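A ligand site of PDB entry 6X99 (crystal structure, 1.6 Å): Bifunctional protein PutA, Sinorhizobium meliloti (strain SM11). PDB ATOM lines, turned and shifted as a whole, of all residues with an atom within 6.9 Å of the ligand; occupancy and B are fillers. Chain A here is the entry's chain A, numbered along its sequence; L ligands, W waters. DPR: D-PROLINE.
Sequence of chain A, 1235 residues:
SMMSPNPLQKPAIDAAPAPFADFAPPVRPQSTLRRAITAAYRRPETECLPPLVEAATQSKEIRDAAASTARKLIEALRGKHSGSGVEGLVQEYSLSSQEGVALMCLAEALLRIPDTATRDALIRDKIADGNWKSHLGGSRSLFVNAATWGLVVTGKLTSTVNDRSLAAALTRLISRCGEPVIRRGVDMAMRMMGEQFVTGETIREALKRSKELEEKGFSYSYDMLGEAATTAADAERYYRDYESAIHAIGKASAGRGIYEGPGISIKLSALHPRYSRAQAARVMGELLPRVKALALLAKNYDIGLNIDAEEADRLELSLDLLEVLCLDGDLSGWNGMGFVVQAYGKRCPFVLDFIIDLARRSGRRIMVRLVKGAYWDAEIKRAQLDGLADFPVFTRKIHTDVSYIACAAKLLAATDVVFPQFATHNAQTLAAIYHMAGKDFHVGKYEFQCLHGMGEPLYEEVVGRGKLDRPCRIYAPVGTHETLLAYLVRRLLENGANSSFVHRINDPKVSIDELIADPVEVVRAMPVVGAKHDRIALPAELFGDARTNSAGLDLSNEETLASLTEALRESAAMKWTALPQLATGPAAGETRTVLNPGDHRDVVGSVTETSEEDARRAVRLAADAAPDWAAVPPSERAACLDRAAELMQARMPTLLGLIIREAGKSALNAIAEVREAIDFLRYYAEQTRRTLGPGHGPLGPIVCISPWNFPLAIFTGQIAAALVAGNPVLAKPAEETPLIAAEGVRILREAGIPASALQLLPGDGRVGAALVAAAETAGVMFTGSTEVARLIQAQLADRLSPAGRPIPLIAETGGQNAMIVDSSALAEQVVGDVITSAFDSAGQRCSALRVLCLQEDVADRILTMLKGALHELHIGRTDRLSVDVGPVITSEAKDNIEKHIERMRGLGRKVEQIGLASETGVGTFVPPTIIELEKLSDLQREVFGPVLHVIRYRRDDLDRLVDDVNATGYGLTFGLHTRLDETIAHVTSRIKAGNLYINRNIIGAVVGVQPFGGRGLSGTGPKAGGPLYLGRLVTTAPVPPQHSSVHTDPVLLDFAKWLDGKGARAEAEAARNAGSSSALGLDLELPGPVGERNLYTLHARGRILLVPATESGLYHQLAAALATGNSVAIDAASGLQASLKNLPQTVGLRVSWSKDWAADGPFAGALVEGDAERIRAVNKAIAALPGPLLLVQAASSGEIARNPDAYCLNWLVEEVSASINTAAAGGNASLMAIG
N of the ligand lies within salt-bridge range of OE2 of Glu 676.
N of Ala 1005 is in hydrogen-bond range of O of the ligand.
The backbone NH (N) of Gly 1004 lies within hydrogen-bond range of an oxygen (O) of the ligand (3.0 Å).
NH1 of Arg 845 is in salt-bridge range of OXT of the ligand.
OG of Ser 847 lies within hydrogen-bond range of O of the ligand (3.1 Å).
CZ of Phe 710 touches OXT of the ligand (3.2 Å).
Ile 714 touches the ligand.
Ile 1003 touches the ligand (C to O, 3.8 Å).
Phe 1012 touches the ligand.
Of the 22 residues printed, 9 come within 4 Å of the ligand.
Along chain A the residues within 4 Å of the ligand span positions 676 to 1012.
The nearest printed residue that does not touch the ligand is Glu 812 (4.9 Å).
The side-chain hydroxyl of Thr 973 sits at hydrogen-bond distance from the backbone carbonyl oxygen of Ser 847 (2.9 Å).
The backbone NH of Phe 1012 lies within hydrogen-bond range of the backbone carbonyl oxygen of Ala 1024.
Water W3 lies within hydrogen-bond range of N of Cys 846, OXT of the ligand and N of Ser 847.
Water W2 lies within hydrogen-bond range of the side-chain hydroxyl (OH) of Tyr 997 (2.7 Å), the backbone carbonyl oxygen (O) of Ile 1002 (2.8 Å) and an oxygen (O) of the ligand (3.0 Å).
Water W1 lies within hydrogen-bond range of the side-chain carboxylate of Glu 812 (3.2 Å) and the side-chain sulfur of Cys 846 (3.5 Å).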
ATOM      1  N   GLU A 676     -28.016  30.208 -27.468  1.00  0.00           N
ATOM      2  CA  GLU A 676     -26.767  30.018 -28.208  1.00  0.00           C
ATOM      3  C   GLU A 676     -26.869  30.593 -29.611  1.00  0.00           C
ATOM      4  O   GLU A 676     -25.917  31.230 -30.103  1.00  0.00           O
ATOM      5  CB  GLU A 676     -26.400  28.534 -28.232  1.00  0.00           C
ATOM      6  CG  GLU A 676     -24.966  28.287 -28.662  1.00  0.00           C
ATOM      7  CD  GLU A 676     -24.519  26.842 -28.455  1.00  0.00           C
ATOM      8  OE1 GLU A 676     -23.359  26.523 -28.795  1.00  0.00           O
ATOM      9  OE2 GLU A 676     -25.329  26.036 -27.967  1.00  0.00           O
ATOM     10  N   PHE A 680     -24.524  33.526 -30.979  1.00  0.00           N
ATOM     11  CA  PHE A 680     -23.724  33.424 -32.196  1.00  0.00           C
ATOM     12  C   PHE A 680     -23.923  34.646 -33.087  1.00  0.00           C
ATOM     13  O   PHE A 680     -22.957  35.257 -33.562  1.00  0.00           O
ATOM     14  CB  PHE A 680     -24.104  32.170 -32.993  1.00  0.00           C
ATOM     15  CG  PHE A 680     -23.385  30.913 -32.568  1.00  0.00           C
ATOM     16  CD1 PHE A 680     -22.019  30.894 -32.379  1.00  0.00           C
ATOM     17  CD2 PHE A 680     -24.108  29.742 -32.411  1.00  0.00           C
ATOM     18  CE1 PHE A 680     -21.357  29.710 -32.012  1.00  0.00           C
ATOM     19  CE2 PHE A 680     -23.477  28.552 -32.038  1.00  0.00           C
ATOM     20  CZ  PHE A 680     -22.085  28.543 -31.839  1.00  0.00           C
ATOM     21  N   ASN A 709     -28.567  17.622 -33.639  1.00  0.00           N
ATOM     22  CA  ASN A 709     -28.507  17.767 -32.196  1.00  0.00           C
ATOM     23  C   ASN A 709     -28.491  19.218 -31.737  1.00  0.00           C
ATOM     24  O   ASN A 709     -28.836  19.486 -30.579  1.00  0.00           O
ATOM     25  CB  ASN A 709     -27.299  17.001 -31.624  1.00  0.00           C
ATOM     26  CG  ASN A 709     -25.962  17.615 -32.029  1.00  0.00           C
ATOM     27  OD1 ASN A 709     -25.870  18.399 -32.969  1.00  0.00           O
ATOM     28  ND2 ASN A 709     -24.902  17.207 -31.320  1.00  0.00           N
ATOM     29  N   PHE A 710     -28.122  20.151 -32.606  1.00  0.00           N
ATOM     30  CA  PHE A 710     -28.262  21.590 -32.363  1.00  0.00           C
ATOM     31  C   PHE A 710     -28.861  22.212 -33.618  1.00  0.00           C
ATOM     32  O   PHE A 710     -28.220  22.998 -34.323  1.00  0.00           O
ATOM     33  CB  PHE A 710     -26.925  22.218 -31.964  1.00  0.00           C
ATOM     34  CG  PHE A 710     -26.532  21.849 -30.583  1.00  0.00           C
ATOM     35  CD1 PHE A 710     -27.057  22.529 -29.501  1.00  0.00           C
ATOM     36  CD2 PHE A 710     -25.710  20.752 -30.357  1.00  0.00           C
ATOM     37  CE1 PHE A 710     -26.732  22.163 -28.218  1.00  0.00           C
ATOM     38  CE2 PHE A 710     -25.393  20.382 -29.063  1.00  0.00           C
ATOM     39  CZ  PHE A 710     -25.911  21.093 -28.000  1.00  0.00           C
ATOM     40  N   ALA A 713     -28.971  26.191 -33.112  1.00  0.00           N
ATOM     41  CA  ALA A 713     -27.794  26.949 -32.691  1.00  0.00           C
ATOM     42  C   ALA A 713     -26.632  26.772 -33.665  1.00  0.00           C
ATOM     43  O   ALA A 713     -26.039  27.755 -34.120  1.00  0.00           O
ATOM     44  CB  ALA A 713     -27.389  26.554 -31.269  1.00  0.00           C
ATOM     45  N   ILE A 714     -26.258  25.529 -33.967  1.00  0.00           N
ATOM     46  CA  ILE A 714     -25.127  25.325 -34.875  1.00  0.00           C
ATOM     47  C   ILE A 714     -25.536  25.635 -36.313  1.00  0.00           C
ATOM     48  O   ILE A 714     -24.731  26.135 -37.103  1.00  0.00           O
ATOM     49  CB  ILE A 714     -24.563  23.899 -34.704  1.00  0.00           C
ATOM     50  CG1 ILE A 714     -23.843  23.800 -33.351  1.00  0.00           C
ATOM     51  CG2 ILE A 714     -23.605  23.569 -35.870  1.00  0.00           C
ATOM     52  CD1 ILE A 714     -23.359  22.406 -32.976  1.00  0.00           C
ATOM     53  N   GLU A 812     -16.325  20.087 -37.491  1.00  0.00           N
ATOM     54  CA  GLU A 812     -16.421  19.715 -36.069  1.00  0.00           C
ATOM     55  C   GLU A 812     -17.019  18.315 -35.974  1.00  0.00           C
ATOM     56  O   GLU A 812     -18.048  18.053 -36.591  1.00  0.00           O
ATOM     57  CB  GLU A 812     -17.294  20.705 -35.283  1.00  0.00           C
ATOM     58  CG  GLU A 812     -17.138  20.700 -33.745  1.00  0.00           C
ATOM     59  CD  GLU A 812     -18.251  19.970 -32.968  1.00  0.00           C
ATOM     60  OE1 GLU A 812     -19.350  20.552 -32.737  1.00  0.00           O
ATOM     61  OE2 GLU A 812     -18.020  18.799 -32.582  1.00  0.00           O
ATOM     62  N   ARG A 845     -25.313  15.547 -27.093  1.00  0.00           N
ATOM     63  CA  ARG A 845     -24.351  16.616 -27.302  1.00  0.00           C
ATOM     64  C   ARG A 845     -23.016  16.039 -27.763  1.00  0.00           C
ATOM     65  O   ARG A 845     -22.576  14.988 -27.280  1.00  0.00           O
ATOM     66  CB  ARG A 845     -24.118  17.411 -26.028  1.00  0.00           C
ATOM     67  CG  ARG A 845     -25.348  18.144 -25.501  1.00  0.00           C
ATOM     68  CD  ARG A 845     -24.984  18.865 -24.229  1.00  0.00           C
ATOM     69  NE  ARG A 845     -26.149  19.496 -23.615  1.00  0.00           N
ATOM     70  CZ  ARG A 845     -26.452  20.781 -23.737  1.00  0.00           C
ATOM     71  NH1 ARG A 845     -25.664  21.599 -24.430  1.00  0.00           N
ATOM     72  NH2 ARG A 845     -27.542  21.256 -23.136  1.00  0.00           N
ATOM     73  N   CYS A 846     -22.367  16.739 -28.683  1.00  0.00           N
ATOM     74  CA  CYS A 846     -20.986  16.357 -28.986  1.00  0.00           C
ATOM     75  C   CYS A 846     -20.088  16.513 -27.772  1.00  0.00           C
ATOM     76  O   CYS A 846     -19.091  15.787 -27.635  1.00  0.00           O
ATOM     77  CB  CYS A 846     -20.456  17.185 -30.144  1.00  0.00           C
ATOM     78  SG  CYS A 846     -21.236  16.650 -31.659  1.00  0.00           S
ATOM     79  N   SER A 847     -20.410  17.458 -26.879  1.00  0.00           N
ATOM     80  CA  SER A 847     -19.653  17.716 -25.666  1.00  0.00           C
ATOM     81  C   SER A 847     -19.968  16.751 -24.528  1.00  0.00           C
ATOM     82  O   SER A 847     -19.380  16.887 -23.450  1.00  0.00           O
ATOM     83  CB  SER A 847     -19.952  19.131 -25.181  1.00  0.00           C
ATOM     84  OG  SER A 847     -21.352  19.288 -25.039  1.00  0.00           O
ATOM     85  N   ALA A 848     -20.885  15.803 -24.720  1.00  0.00           N
ATOM     86  CA  ALA A 848     -21.384  14.988 -23.626  1.00  0.00           C
ATOM     87  C   ALA A 848     -20.283  14.133 -23.004  1.00  0.00           C
ATOM     88  O   ALA A 848     -19.384  13.652 -23.684  1.00  0.00           O
ATOM     89  CB  ALA A 848     -22.519  14.083 -24.127  1.00  0.00           C
ATOM     90  N   THR A 973     -14.171  17.921 -25.426  1.00  0.00           N
ATOM     91  CA  THR A 973     -14.347  18.409 -24.073  1.00  0.00           C
ATOM     92  C   THR A 973     -13.675  17.461 -23.083  1.00  0.00           C
ATOM     93  O   THR A 973     -13.474  16.273 -23.346  1.00  0.00           O
ATOM     94  CB  THR A 973     -15.839  18.570 -23.692  1.00  0.00           C
ATOM     95  OG1 THR A 973     -16.500  17.314 -23.804  1.00  0.00           O
ATOM     96  CG2 THR A 973     -16.552  19.609 -24.588  1.00  0.00           C
ATOM     97  N   TYR A 997     -12.819  21.893 -18.504  1.00  0.00           N
ATOM     98  CA  TYR A 997     -13.790  22.296 -17.508  1.00  0.00           C
ATOM     99  C   TYR A 997     -13.314  21.788 -16.155  1.00  0.00           C
ATOM    100  O   TYR A 997     -13.095  20.587 -15.991  1.00  0.00           O
ATOM    101  CB  TYR A 997     -15.170  21.737 -17.837  1.00  0.00           C
ATOM    102  CG  TYR A 997     -15.733  22.306 -19.125  1.00  0.00           C
ATOM    103  CD1 TYR A 997     -16.326  23.558 -19.153  1.00  0.00           C
ATOM    104  CD2 TYR A 997     -15.671  21.577 -20.314  1.00  0.00           C
ATOM    105  CE1 TYR A 997     -16.857  24.087 -20.317  1.00  0.00           C
ATOM    106  CE2 TYR A 997     -16.208  22.103 -21.491  1.00  0.00           C
ATOM    107  CZ  TYR A 997     -16.788  23.356 -21.486  1.00  0.00           C
ATOM    108  OH  TYR A 997     -17.315  23.888 -22.637  1.00  0.00           O
ATOM    109  N   ILE A1002     -19.269  19.604 -18.196  1.00  0.00           N
ATOM    110  CA  ILE A1002     -18.495  19.794 -19.417  1.00  0.00           C
ATOM    111  C   ILE A1002     -19.376  20.148 -20.607  1.00  0.00           C
ATOM    112  O   ILE A1002     -18.929  20.075 -21.746  1.00  0.00           O
ATOM    113  CB  ILE A1002     -17.609  18.555 -19.728  1.00  0.00           C
ATOM    114  CG1 ILE A1002     -18.451  17.339 -20.163  1.00  0.00           C
ATOM    115  CG2 ILE A1002     -16.733  18.219 -18.525  1.00  0.00           C
ATOM    116  CD1 ILE A1002     -17.565  16.140 -20.571  1.00  0.00           C
ATOM    117  N   ILE A1003     -20.617  20.585 -20.374  1.00  0.00           N
ATOM    118  CA  ILE A1003     -21.541  20.809 -21.475  1.00  0.00           C
ATOM    119  C   ILE A1003     -21.998  22.271 -21.510  1.00  0.00           C
ATOM    120  O   ILE A1003     -21.755  23.048 -20.580  1.00  0.00           O
ATOM    121  CB  ILE A1003     -22.772  19.883 -21.422  1.00  0.00           C
ATOM    122  CG1 ILE A1003     -23.579  20.077 -20.132  1.00  0.00           C
ATOM    123  CG2 ILE A1003     -22.368  18.435 -21.643  1.00  0.00           C
ATOM    124  CD1 ILE A1003     -24.979  19.425 -20.232  1.00  0.00           C
ATOM    125  N   GLY A1004     -22.680  22.615 -22.597  1.00  0.00           N
ATOM    126  CA  GLY A1004     -23.249  23.949 -22.727  1.00  0.00           C
ATOM    127  C   GLY A1004     -22.217  25.057 -22.873  1.00  0.00           C
ATOM    128  O   GLY A1004     -22.379  26.122 -22.272  1.00  0.00           O
ATOM    129  N   ALA A1005     -21.180  24.828 -23.682  1.00  0.00           N
ATOM    130  CA  ALA A1005     -20.217  25.869 -23.994  1.00  0.00           C
ATOM    131  C   ALA A1005     -20.948  27.132 -24.425  1.00  0.00           C
ATOM    132  O   ALA A1005     -21.913  27.081 -25.186  1.00  0.00           O
ATOM    133  CB  ALA A1005     -19.276  25.413 -25.113  1.00  0.00           C
ATOM    134  N   VAL A1006     -20.487  28.272 -23.897  1.00  0.00           N
ATOM    135  CA  VAL A1006     -21.140  29.559 -24.067  1.00  0.00           C
ATOM    136  C   VAL A1006     -20.347  30.364 -25.088  1.00  0.00           C
ATOM    137  O   VAL A1006     -19.132  30.536 -24.952  1.00  0.00           O
ATOM    138  CB  VAL A1006     -21.231  30.312 -22.731  1.00  0.00           C
ATOM    139  CG1 VAL A1006     -21.647  31.749 -22.941  1.00  0.00           C
ATOM    140  CG2 VAL A1006     -22.207  29.595 -21.793  1.00  0.00           C
ATOM    141  N   GLN A1010     -16.724  30.265 -23.571  1.00  0.00           N
ATOM    142  CA  GLN A1010     -15.990  29.053 -23.892  1.00  0.00           C
ATOM    143  C   GLN A1010     -16.111  28.842 -25.394  1.00  0.00           C
ATOM    144  O   GLN A1010     -16.931  28.043 -25.853  1.00  0.00           O
ATOM    145  CB  GLN A1010     -16.504  27.835 -23.132  1.00  0.00           C
ATOM    146  CG  GLN A1010     -16.482  27.991 -21.622  1.00  0.00           C
ATOM    147  CD  GLN A1010     -17.832  28.388 -21.038  1.00  0.00           C
ATOM    148  OE1 GLN A1010     -18.893  28.045 -21.575  1.00  0.00           O
ATOM    149  NE2 GLN A1010     -17.792  29.127 -19.923  1.00  0.00           N
ATOM    150  N   PHE A1012     -15.781  27.111 -28.670  1.00  0.00           N
ATOM    151  CA  PHE A1012     -15.987  25.673 -28.634  1.00  0.00           C
ATOM    152  C   PHE A1012     -15.359  25.009 -29.848  1.00  0.00           C
ATOM    153  O   PHE A1012     -15.604  25.427 -30.988  1.00  0.00           O
ATOM    154  CB  PHE A1012     -17.472  25.344 -28.590  1.00  0.00           C
ATOM    155  CG  PHE A1012     -17.735  23.891 -28.473  1.00  0.00           C
ATOM    156  CD1 PHE A1012     -17.577  23.255 -27.248  1.00  0.00           C
ATOM    157  CD2 PHE A1012     -18.107  23.146 -29.587  1.00  0.00           C
ATOM    158  CE1 PHE A1012     -17.817  21.898 -27.126  1.00  0.00           C
ATOM    159  CE2 PHE A1012     -18.338  21.789 -29.468  1.00  0.00           C
ATOM    160  CZ  PHE A1012     -18.197  21.163 -28.232  1.00  0.00           C
ATOM    161  N   GLY A1013     -14.615  23.952 -29.610  1.00  0.00           N
ATOM    162  CA  GLY A1013     -14.025  23.197 -30.698  1.00  0.00           C
ATOM    163  C   GLY A1013     -12.749  22.540 -30.236  1.00  0.00           C
ATOM    164  O   GLY A1013     -12.028  23.040 -29.386  1.00  0.00           O
ATOM    165  N   ALA A1024     -15.816  27.569 -32.992  1.00  0.00           N
ATOM    166  CA  ALA A1024     -17.049  28.330 -33.083  1.00  0.00           C
ATOM    167  C   ALA A1024     -17.201  29.208 -31.857  1.00  0.00           C
ATOM    168  O   ALA A1024     -16.822  28.821 -30.739  1.00  0.00           O
ATOM    169  CB  ALA A1024     -18.238  27.375 -33.196  1.00  0.00           C
HETATM  170  N   DPR L   1     -23.682  23.655 -27.915  1.00  0.00           N
HETATM  171  CA  DPR L   1     -22.497  23.670 -27.014  1.00  0.00           C
HETATM  172  CB  DPR L   1     -21.239  23.725 -27.907  1.00  0.00           C
HETATM  173  CG  DPR L   1     -21.691  23.010 -29.185  1.00  0.00           C
HETATM  174  CD  DPR L   1     -23.202  23.368 -29.309  1.00  0.00           C
HETATM  175  C   DPR L   1     -22.401  22.397 -26.099  1.00  0.00           C
HETATM  176  O   DPR L   1     -21.460  22.359 -25.290  1.00  0.00           O
HETATM  177  OXT DPR L   1     -23.291  21.535 -26.271  1.00  0.00           O
HETATM  178  O   HOH W   1     -21.816  20.017 -30.757  1.00  0.00           O
HETATM  179  O   HOH W   2     -18.942  22.009 -23.736  1.00  0.00           O
HETATM  180  O   HOH W   3     -22.175  19.623 -28.253  1.00  0.00           O
